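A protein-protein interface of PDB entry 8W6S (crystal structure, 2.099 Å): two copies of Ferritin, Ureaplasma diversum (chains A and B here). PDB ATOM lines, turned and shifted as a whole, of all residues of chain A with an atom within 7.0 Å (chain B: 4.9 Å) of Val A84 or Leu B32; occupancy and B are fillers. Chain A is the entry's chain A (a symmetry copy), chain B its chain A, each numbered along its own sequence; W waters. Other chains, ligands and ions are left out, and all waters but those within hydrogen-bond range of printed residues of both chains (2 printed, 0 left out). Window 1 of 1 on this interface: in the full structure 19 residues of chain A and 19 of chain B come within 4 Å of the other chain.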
ATOM      1  N   TYR A  24       9.089 -22.526 -26.917  1.00  0.00           N
ATOM      2  CA  TYR A  24       9.464 -21.228 -26.366  1.00  0.00           C
ATOM      3  C   TYR A  24       8.223 -20.420 -26.015  1.00  0.00           C
ATOM      4  O   TYR A  24       8.079 -19.920 -24.891  1.00  0.00           O
ATOM      5  CB  TYR A  24      10.339 -20.484 -27.386  1.00  0.00           C
ATOM      6  CG  TYR A  24      10.877 -19.136 -26.949  1.00  0.00           C
ATOM      7  CD1 TYR A  24      10.119 -17.975 -27.100  1.00  0.00           C
ATOM      8  CD2 TYR A  24      12.159 -19.019 -26.420  1.00  0.00           C
ATOM      9  CE1 TYR A  24      10.614 -16.741 -26.721  1.00  0.00           C
ATOM     10  CE2 TYR A  24      12.658 -17.792 -26.022  1.00  0.00           C
ATOM     11  CZ  TYR A  24      11.880 -16.658 -26.172  1.00  0.00           C
ATOM     12  OH  TYR A  24      12.383 -15.440 -25.783  1.00  0.00           O
ATOM     13  N   LYS A  25       7.313 -20.292 -26.983  1.00  0.00           N
ATOM     14  CA  LYS A  25       6.021 -19.643 -26.784  1.00  0.00           C
ATOM     15  C   LYS A  25       5.267 -20.237 -25.591  1.00  0.00           C
ATOM     16  O   LYS A  25       4.731 -19.511 -24.742  1.00  0.00           O
ATOM     17  CB  LYS A  25       5.215 -19.796 -28.079  1.00  0.00           C
ATOM     18  CG  LYS A  25       3.776 -19.281 -28.076  1.00  0.00           C
ATOM     19  CD  LYS A  25       3.182 -19.446 -29.489  1.00  0.00           C
ATOM     20  CE  LYS A  25       1.671 -19.317 -29.484  1.00  0.00           C
ATOM     21  NZ  LYS A  25       1.292 -17.878 -29.486  1.00  0.00           N
ATOM     22  N   VAL A  28       6.810 -19.120 -22.260  1.00  0.00           N
ATOM     23  CA  VAL A  28       6.493 -17.719 -21.981  1.00  0.00           C
ATOM     24  C   VAL A  28       5.058 -17.590 -21.478  1.00  0.00           C
ATOM     25  O   VAL A  28       4.800 -17.028 -20.406  1.00  0.00           O
ATOM     26  CB  VAL A  28       6.721 -16.857 -23.236  1.00  0.00           C
ATOM     27  CG1 VAL A  28       6.077 -15.482 -23.049  1.00  0.00           C
ATOM     28  CG2 VAL A  28       8.200 -16.746 -23.544  1.00  0.00           C
ATOM     29  N   GLU A  29       4.103 -18.115 -22.251  1.00  0.00           N
ATOM     30  CA  GLU A  29       2.695 -17.950 -21.910  1.00  0.00           C
ATOM     31  C   GLU A  29       2.356 -18.645 -20.598  1.00  0.00           C
ATOM     32  O   GLU A  29       1.664 -18.071 -19.747  1.00  0.00           O
ATOM     33  CB  GLU A  29       1.821 -18.455 -23.070  1.00  0.00           C
ATOM     34  CG  GLU A  29       2.048 -17.573 -24.306  1.00  0.00           C
ATOM     35  CD  GLU A  29       1.341 -18.026 -25.567  1.00  0.00           C
ATOM     36  OE1 GLU A  29       1.409 -17.256 -26.546  1.00  0.00           O
ATOM     37  OE2 GLU A  29       0.730 -19.120 -25.594  1.00  0.00           O
ATOM     38  N   LEU A  32       3.505 -16.537 -17.753  1.00  0.00           N
ATOM     39  CA  LEU A  32       2.632 -15.396 -17.487  1.00  0.00           C
ATOM     40  C   LEU A  32       1.351 -15.828 -16.789  1.00  0.00           C
ATOM     41  O   LEU A  32       0.855 -15.125 -15.894  1.00  0.00           O
ATOM     42  CB  LEU A  32       2.320 -14.656 -18.789  1.00  0.00           C
ATOM     43  CG  LEU A  32       3.537 -13.973 -19.437  1.00  0.00           C
ATOM     44  CD1 LEU A  32       3.253 -13.476 -20.865  1.00  0.00           C
ATOM     45  CD2 LEU A  32       4.017 -12.827 -18.553  1.00  0.00           C
ATOM     46  N   LEU A  62       9.720 -18.666 -17.424  1.00  0.00           N
ATOM     47  CA  LEU A  62      10.157 -17.454 -18.106  1.00  0.00           C
ATOM     48  C   LEU A  62      11.657 -17.238 -18.010  1.00  0.00           C
ATOM     49  O   LEU A  62      12.163 -16.271 -18.589  1.00  0.00           O
ATOM     50  CB  LEU A  62       9.427 -16.241 -17.533  1.00  0.00           C
ATOM     51  CG  LEU A  62       7.994 -15.961 -17.981  1.00  0.00           C
ATOM     52  CD1 LEU A  62       7.321 -15.044 -16.980  1.00  0.00           C
ATOM     53  CD2 LEU A  62       8.013 -15.319 -19.360  1.00  0.00           C
ATOM     54  N   LYS A  66      13.010 -20.880 -21.229  1.00  0.00           N
ATOM     55  CA  LYS A  66      13.072 -20.189 -22.512  1.00  0.00           C
ATOM     56  C   LYS A  66      14.491 -19.792 -22.889  1.00  0.00           C
ATOM     57  O   LYS A  66      14.829 -19.791 -24.081  1.00  0.00           O
ATOM     58  CB  LYS A  66      12.153 -18.953 -22.504  1.00  0.00           C
ATOM     59  CG  LYS A  66      12.796 -17.606 -22.076  1.00  0.00           C
ATOM     60  CD  LYS A  66      11.752 -16.492 -22.043  1.00  0.00           C
ATOM     61  CE  LYS A  66      12.393 -15.101 -22.009  1.00  0.00           C
ATOM     62  NZ  LYS A  66      13.280 -14.941 -20.844  1.00  0.00           N
ATOM     63  N   LYS A  81      11.596 -16.955 -32.922  1.00  0.00           N
ATOM     64  CA  LYS A  81      10.383 -16.188 -33.150  1.00  0.00           C
ATOM     65  C   LYS A  81       9.764 -15.823 -31.810  1.00  0.00           C
ATOM     66  O   LYS A  81       9.635 -16.678 -30.929  1.00  0.00           O
ATOM     67  CB  LYS A  81       9.387 -16.966 -34.015  1.00  0.00           C
ATOM     68  CG  LYS A  81       9.912 -17.195 -35.428  1.00  0.00           C
ATOM     69  CD  LYS A  81       8.805 -17.477 -36.428  1.00  0.00           C
ATOM     70  CE  LYS A  81       9.229 -18.568 -37.408  1.00  0.00           C
ATOM     71  NZ  LYS A  81       8.100 -18.993 -38.287  1.00  0.00           N
ATOM     72  N   THR A  82       9.389 -14.555 -31.657  1.00  0.00           N
ATOM     73  CA  THR A  82       8.607 -14.105 -30.506  1.00  0.00           C
ATOM     74  C   THR A  82       7.205 -13.763 -30.981  1.00  0.00           C
ATOM     75  O   THR A  82       7.011 -12.775 -31.698  1.00  0.00           O
ATOM     76  CB  THR A  82       9.261 -12.911 -29.807  1.00  0.00           C
ATOM     77  OG1 THR A  82      10.542 -13.307 -29.310  1.00  0.00           O
ATOM     78  CG2 THR A  82       8.395 -12.401 -28.654  1.00  0.00           C
ATOM     79  N   ASP A  83       6.229 -14.573 -30.557  1.00  0.00           N
ATOM     80  CA  ASP A  83       4.828 -14.370 -30.933  1.00  0.00           C
ATOM     81  C   ASP A  83       3.966 -14.875 -29.774  1.00  0.00           C
ATOM     82  O   ASP A  83       3.744 -16.081 -29.636  1.00  0.00           O
ATOM     83  CB  ASP A  83       4.500 -15.085 -32.240  1.00  0.00           C
ATOM     84  CG  ASP A  83       3.077 -14.837 -32.689  1.00  0.00           C
ATOM     85  OD1 ASP A  83       2.414 -13.974 -32.079  1.00  0.00           O
ATOM     86  OD2 ASP A  83       2.626 -15.486 -33.651  1.00  0.00           O
ATOM     87  N   VAL A  84       3.473 -13.947 -28.959  1.00  0.00           N
ATOM     88  CA  VAL A  84       2.942 -14.269 -27.642  1.00  0.00           C
ATOM     89  C   VAL A  84       1.546 -13.689 -27.515  1.00  0.00           C
ATOM     90  O   VAL A  84       1.349 -12.486 -27.720  1.00  0.00           O
ATOM     91  CB  VAL A  84       3.851 -13.716 -26.529  1.00  0.00           C
ATOM     92  CG1 VAL A  84       3.180 -13.834 -25.167  1.00  0.00           C
ATOM     93  CG2 VAL A  84       5.207 -14.417 -26.555  1.00  0.00           C
ATOM     94  N   SER A  85       0.588 -14.531 -27.155  1.00  0.00           N
ATOM     95  CA  SER A  85      -0.756 -14.067 -26.848  1.00  0.00           C
ATOM     96  C   SER A  85      -1.319 -14.924 -25.727  1.00  0.00           C
ATOM     97  O   SER A  85      -1.472 -16.137 -25.893  1.00  0.00           O
ATOM     98  CB  SER A  85      -1.654 -14.125 -28.085  1.00  0.00           C
ATOM     99  OG  SER A  85      -2.053 -15.438 -28.382  1.00  0.00           O
ATOM    100  N   VAL A  86      -1.622 -14.307 -24.590  1.00  0.00           N
ATOM    101  CA  VAL A  86      -2.269 -15.045 -23.520  1.00  0.00           C
ATOM    102  C   VAL A  86      -3.065 -14.075 -22.658  1.00  0.00           C
ATOM    103  O   VAL A  86      -2.603 -12.980 -22.333  1.00  0.00           O
ATOM    104  CB  VAL A  86      -1.236 -15.863 -22.710  1.00  0.00           C
ATOM    105  CG1 VAL A  86      -0.138 -14.959 -22.105  1.00  0.00           C
ATOM    106  CG2 VAL A  86      -1.936 -16.720 -21.653  1.00  0.00           C
ATOM    107  N   VAL B  28       5.475  -6.289 -19.209  1.00  0.00           N
ATOM    108  CA  VAL B  28       5.557  -7.662 -19.709  1.00  0.00           C
ATOM    109  C   VAL B  28       5.957  -7.668 -21.181  1.00  0.00           C
ATOM    110  O   VAL B  28       6.934  -8.315 -21.580  1.00  0.00           O
ATOM    111  CB  VAL B  28       4.220  -8.392 -19.494  1.00  0.00           C
ATOM    112  CG1 VAL B  28       4.195  -9.688 -20.307  1.00  0.00           C
ATOM    113  CG2 VAL B  28       3.985  -8.651 -18.020  1.00  0.00           C
ATOM    114  N   GLU B  29       5.203  -6.940 -22.010  1.00  0.00           N
ATOM    115  CA  GLU B  29       5.440  -6.967 -23.449  1.00  0.00           C
ATOM    116  C   GLU B  29       6.807  -6.394 -23.797  1.00  0.00           C
ATOM    117  O   GLU B  29       7.538  -6.972 -24.611  1.00  0.00           O
ATOM    118  CB  GLU B  29       4.304  -6.223 -24.171  1.00  0.00           C
ATOM    119  CG  GLU B  29       2.983  -6.975 -23.961  1.00  0.00           C
ATOM    120  CD  GLU B  29       1.749  -6.292 -24.517  1.00  0.00           C
ATOM    121  OE1 GLU B  29       0.688  -6.944 -24.469  1.00  0.00           O
ATOM    122  OE2 GLU B  29       1.826  -5.134 -24.992  1.00  0.00           O
ATOM    123  N   LEU B  30       7.176  -5.271 -23.177  1.00  0.00           N
ATOM    124  CA  LEU B  30       8.520  -4.732 -23.357  1.00  0.00           C
ATOM    125  C   LEU B  30       9.569  -5.778 -23.007  1.00  0.00           C
ATOM    126  O   LEU B  30      10.528  -5.996 -23.759  1.00  0.00           O
ATOM    127  CB  LEU B  30       8.706  -3.491 -22.480  1.00  0.00           C
ATOM    128  CG  LEU B  30       8.836  -2.094 -23.077  1.00  0.00           C
ATOM    129  CD1 LEU B  30       9.515  -1.199 -22.045  1.00  0.00           C
ATOM    130  CD2 LEU B  30       9.607  -2.120 -24.388  1.00  0.00           C
ATOM    131  N   GLY B  31       9.395  -6.437 -21.856  1.00  0.00           N
ATOM    132  CA  GLY B  31      10.350  -7.449 -21.438  1.00  0.00           C
ATOM    133  C   GLY B  31      10.526  -8.539 -22.472  1.00  0.00           C
ATOM    134  O   GLY B  31      11.647  -8.999 -22.719  1.00  0.00           O
ATOM    135  N   LEU B  32       9.426  -8.948 -23.111  1.00  0.00           N
ATOM    136  CA  LEU B  32       9.497  -9.995 -24.129  1.00  0.00           C
ATOM    137  C   LEU B  32      10.169  -9.490 -25.398  1.00  0.00           C
ATOM    138  O   LEU B  32      10.938 -10.226 -26.036  1.00  0.00           O
ATOM    139  CB  LEU B  32       8.096 -10.531 -24.432  1.00  0.00           C
ATOM    140  CG  LEU B  32       7.438 -11.280 -23.260  1.00  0.00           C
ATOM    141  CD1 LEU B  32       5.945 -11.567 -23.497  1.00  0.00           C
ATOM    142  CD2 LEU B  32       8.197 -12.573 -22.983  1.00  0.00           C
ATOM    143  N   VAL B  33       9.904  -8.235 -25.774  1.00  0.00           N
ATOM    144  CA  VAL B  33      10.592  -7.646 -26.920  1.00  0.00           C
ATOM    145  C   VAL B  33      12.084  -7.565 -26.646  1.00  0.00           C
ATOM    146  O   VAL B  33      12.915  -7.915 -27.493  1.00  0.00           O
ATOM    147  CB  VAL B  33      10.012  -6.258 -27.254  1.00  0.00           C
ATOM    148  CG1 VAL B  33      10.874  -5.559 -28.311  1.00  0.00           C
ATOM    149  CG2 VAL B  33       8.576  -6.386 -27.732  1.00  0.00           C
ATOM    150  N   TYR B  34      12.448  -7.093 -25.457  1.00  0.00           N
ATOM    151  CA  TYR B  34      13.867  -6.993 -25.129  1.00  0.00           C
ATOM    152  C   TYR B  34      14.548  -8.363 -25.137  1.00  0.00           C
ATOM    153  O   TYR B  34      15.696  -8.486 -25.580  1.00  0.00           O
ATOM    154  CB  TYR B  34      14.043  -6.304 -23.786  1.00  0.00           C
ATOM    155  CG  TYR B  34      13.712  -4.837 -23.795  1.00  0.00           C
ATOM    156  CD1 TYR B  34      13.541  -4.140 -24.989  1.00  0.00           C
ATOM    157  CD2 TYR B  34      13.601  -4.136 -22.608  1.00  0.00           C
ATOM    158  CE1 TYR B  34      13.243  -2.782 -24.992  1.00  0.00           C
ATOM    159  CE2 TYR B  34      13.317  -2.786 -22.600  1.00  0.00           C
ATOM    160  CZ  TYR B  34      13.145  -2.109 -23.783  1.00  0.00           C
ATOM    161  OH  TYR B  34      12.856  -0.760 -23.742  1.00  0.00           O
ATOM    162  N   ALA B  35      13.859  -9.410 -24.666  1.00  0.00           N
ATOM    163  CA  ALA B  35      14.453 -10.743 -24.740  1.00  0.00           C
ATOM    164  C   ALA B  35      14.774 -11.105 -26.185  1.00  0.00           C
ATOM    165  O   ALA B  35      15.823 -11.687 -26.471  1.00  0.00           O
ATOM    166  CB  ALA B  35      13.526 -11.796 -24.124  1.00  0.00           C
ATOM    167  N   HIS B  36      13.887 -10.744 -27.114  1.00  0.00           N
ATOM    168  CA  HIS B  36      14.157 -11.009 -28.522  1.00  0.00           C
ATOM    169  C   HIS B  36      15.321 -10.162 -29.014  1.00  0.00           C
ATOM    170  O   HIS B  36      16.252 -10.676 -29.644  1.00  0.00           O
ATOM    171  CB  HIS B  36      12.915 -10.737 -29.369  1.00  0.00           C
ATOM    172  CG  HIS B  36      12.972 -11.382 -30.713  1.00  0.00           C
ATOM    173  ND1 HIS B  36      13.726 -10.867 -31.749  1.00  0.00           N
ATOM    174  CD2 HIS B  36      12.400 -12.512 -31.186  1.00  0.00           C
ATOM    175  CE1 HIS B  36      13.606 -11.651 -32.804  1.00  0.00           C
ATOM    176  NE2 HIS B  36      12.809 -12.659 -32.489  1.00  0.00           N
ATOM    177  N   SER B  58      15.588  -6.735 -20.030  1.00  0.00           N
ATOM    178  CA  SER B  58      14.390  -7.568 -20.184  1.00  0.00           C
ATOM    179  C   SER B  58      13.953  -8.177 -18.849  1.00  0.00           C
ATOM    180  O   SER B  58      12.765  -8.172 -18.506  1.00  0.00           O
ATOM    181  CB  SER B  58      14.649  -8.670 -21.216  1.00  0.00           C
ATOM    182  OG  SER B  58      13.697  -9.718 -21.097  1.00  0.00           O
ATOM    183  N   LEU B  62      10.374  -7.670 -16.729  1.00  0.00           N
ATOM    184  CA  LEU B  62       9.571  -8.838 -16.390  1.00  0.00           C
ATOM    185  C   LEU B  62       9.725  -9.250 -14.936  1.00  0.00           C
ATOM    186  O   LEU B  62       9.059 -10.199 -14.508  1.00  0.00           O
ATOM    187  CB  LEU B  62       9.945 -10.009 -17.297  1.00  0.00           C
ATOM    188  CG  LEU B  62       9.384 -10.052 -18.716  1.00  0.00           C
ATOM    189  CD1 LEU B  62      10.222 -10.989 -19.563  1.00  0.00           C
ATOM    190  CD2 LEU B  62       7.939 -10.524 -18.674  1.00  0.00           C
ATOM    191  N   VAL B  84      -2.000 -10.179 -22.641  1.00  0.00           N
ATOM    192  CA  VAL B  84      -0.685  -9.950 -23.224  1.00  0.00           C
ATOM    193  C   VAL B  84      -0.712 -10.361 -24.683  1.00  0.00           C
ATOM    194  O   VAL B  84      -1.078 -11.498 -25.005  1.00  0.00           O
ATOM    195  CB  VAL B  84       0.400 -10.740 -22.468  1.00  0.00           C
ATOM    196  CG1 VAL B  84       1.725 -10.699 -23.217  1.00  0.00           C
ATOM    197  CG2 VAL B  84       0.540 -10.216 -21.041  1.00  0.00           C
ATOM    198  N   SER B  85      -0.305  -9.453 -25.559  1.00  0.00           N
ATOM    199  CA  SER B  85      -0.136  -9.778 -26.967  1.00  0.00           C
ATOM    200  C   SER B  85       1.050  -8.995 -27.505  1.00  0.00           C
ATOM    201  O   SER B  85       1.030  -7.762 -27.502  1.00  0.00           O
ATOM    202  CB  SER B  85      -1.405  -9.463 -27.761  1.00  0.00           C
ATOM    203  OG  SER B  85      -1.557  -8.084 -27.981  1.00  0.00           O
ATOM    204  N   VAL B  86       2.082  -9.699 -27.959  1.00  0.00           N
ATOM    205  CA  VAL B  86       3.197  -9.016 -28.591  1.00  0.00           C
ATOM    206  C   VAL B  86       3.883  -9.973 -29.555  1.00  0.00           C
ATOM    207  O   VAL B  86       4.095 -11.148 -29.250  1.00  0.00           O
ATOM    208  CB  VAL B  86       4.161  -8.435 -27.529  1.00  0.00           C
ATOM    209  CG1 VAL B  86       4.710  -9.535 -26.592  1.00  0.00           C
ATOM    210  CG2 VAL B  86       5.276  -7.628 -28.198  1.00  0.00           C
ATOM    211  N   ALA B  87       4.198  -9.468 -30.742  1.00  0.00           N
ATOM    212  CA  ALA B  87       4.931 -10.220 -31.748  1.00  0.00           C
ATOM    213  C   ALA B  87       6.039  -9.331 -32.287  1.00  0.00           C
ATOM    214  O   ALA B  87       5.818  -8.145 -32.550  1.00  0.00           O
ATOM    215  CB  ALA B  87       4.017 -10.690 -32.886  1.00  0.00           C
HETATM  216  O   HOH W   1      11.095 -13.149 -26.674  1.00  0.00           O
HETATM  217  O   HOH W   2      13.749 -12.242 -20.183  1.00  0.00           O
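Printed residues of chain B that touch a printed residue of chain A: Val B28, Leu B32, His B36, Val B84, Ser B85, Val B86 and Ala B87. Printed residues of chain A that touch a printed residue of chain B: Val A28, Leu A32, Thr A82, Asp A83, Val A84, Ser A85 and Val A86.
O of Val A86 is in hydrogen-bond range of N of Val B84 (2.9 Å). The backbone carbonyl oxygen (O) of Val B86 sits at hydrogen-bond distance from the backbone NH (N) of Val A84, 2.9 Å away.
Water W2 bridges OG of Ser B58 (2.7 Å) and NZ of Lys A66 (2.8 Å). Water W1 lies within hydrogen-bond range of OG1 of Thr A82 (2.7 Å), OH of Tyr A24 (2.8 Å) and O of Leu B32 (3.0 Å).
Among the printed residues, pairs that only touch across the chains: Thr A82 with His B36 (2.8 Å), Ser A85 with Val B84 (3.2 Å), Val A84 with Ser B85 (3.2 Å), Thr A82 with Ala B87 (3.3 Å), Val A28 with Leu B32 (3.6 Å), Leu A32 with Val B28 (3.6 Å), Asp A83 with Val B86 (3.7 Å), Asp A83 with Ala B87 (3.7 Å), Val A84 with Val B84 (3.8 Å), Val A84 with Leu B32 (3.9 Å) and Leu A32 with Val B84 (3.9 Å).
The side-chain carboxylate (OE1) of Glu B29 is in hydrogen-bond range of the backbone NH (N) of Ser B85 (2.9 Å). O of Asp A83 sits at hydrogen-bond distance from NZ of Lys A25, at 3.0 Å. The side-chain carboxylate (OE1) of Glu A29 is in hydrogen-bond range of the backbone NH (N) of Ser A85 (2.9 Å).
Printed residues of chain A within 4 Å of Leu B32: Val A28 and Val A84. Of the printed residues of chain B, Ser A85 touches Val B84 (3.2 Å). Printed residues of chain A within 4 Å of Ser B85: Val A84. Printed residues of chain B within 4 Å of Val A86: Val B84 (2.9 Å). Of the printed residues of chain B, Val A28 touches Leu B32 (3.6 Å). Lys A81 touches none of the printed residues of chain B. The nearest printed residue of chain B that does not touch Val A84 is Ala B87 (4.9 Å). The nearest printed residue of chain A that does not touch Leu B32 is Leu A32 (4.2 Å).
Val A28 touches Leu B32, and with the chains exchanged Leu A32 touches Val B28. Leu A32 touches Val B84, and with the chains exchanged Val A84 touches Leu B32. Val A84 touches its own counterpart, Val B84. Val A84 touches Val B86, and with the chains exchanged Val A86 touches Val B84. Positions printed for both chains: 28, 29, 32, 62, 84, 85 and 86.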
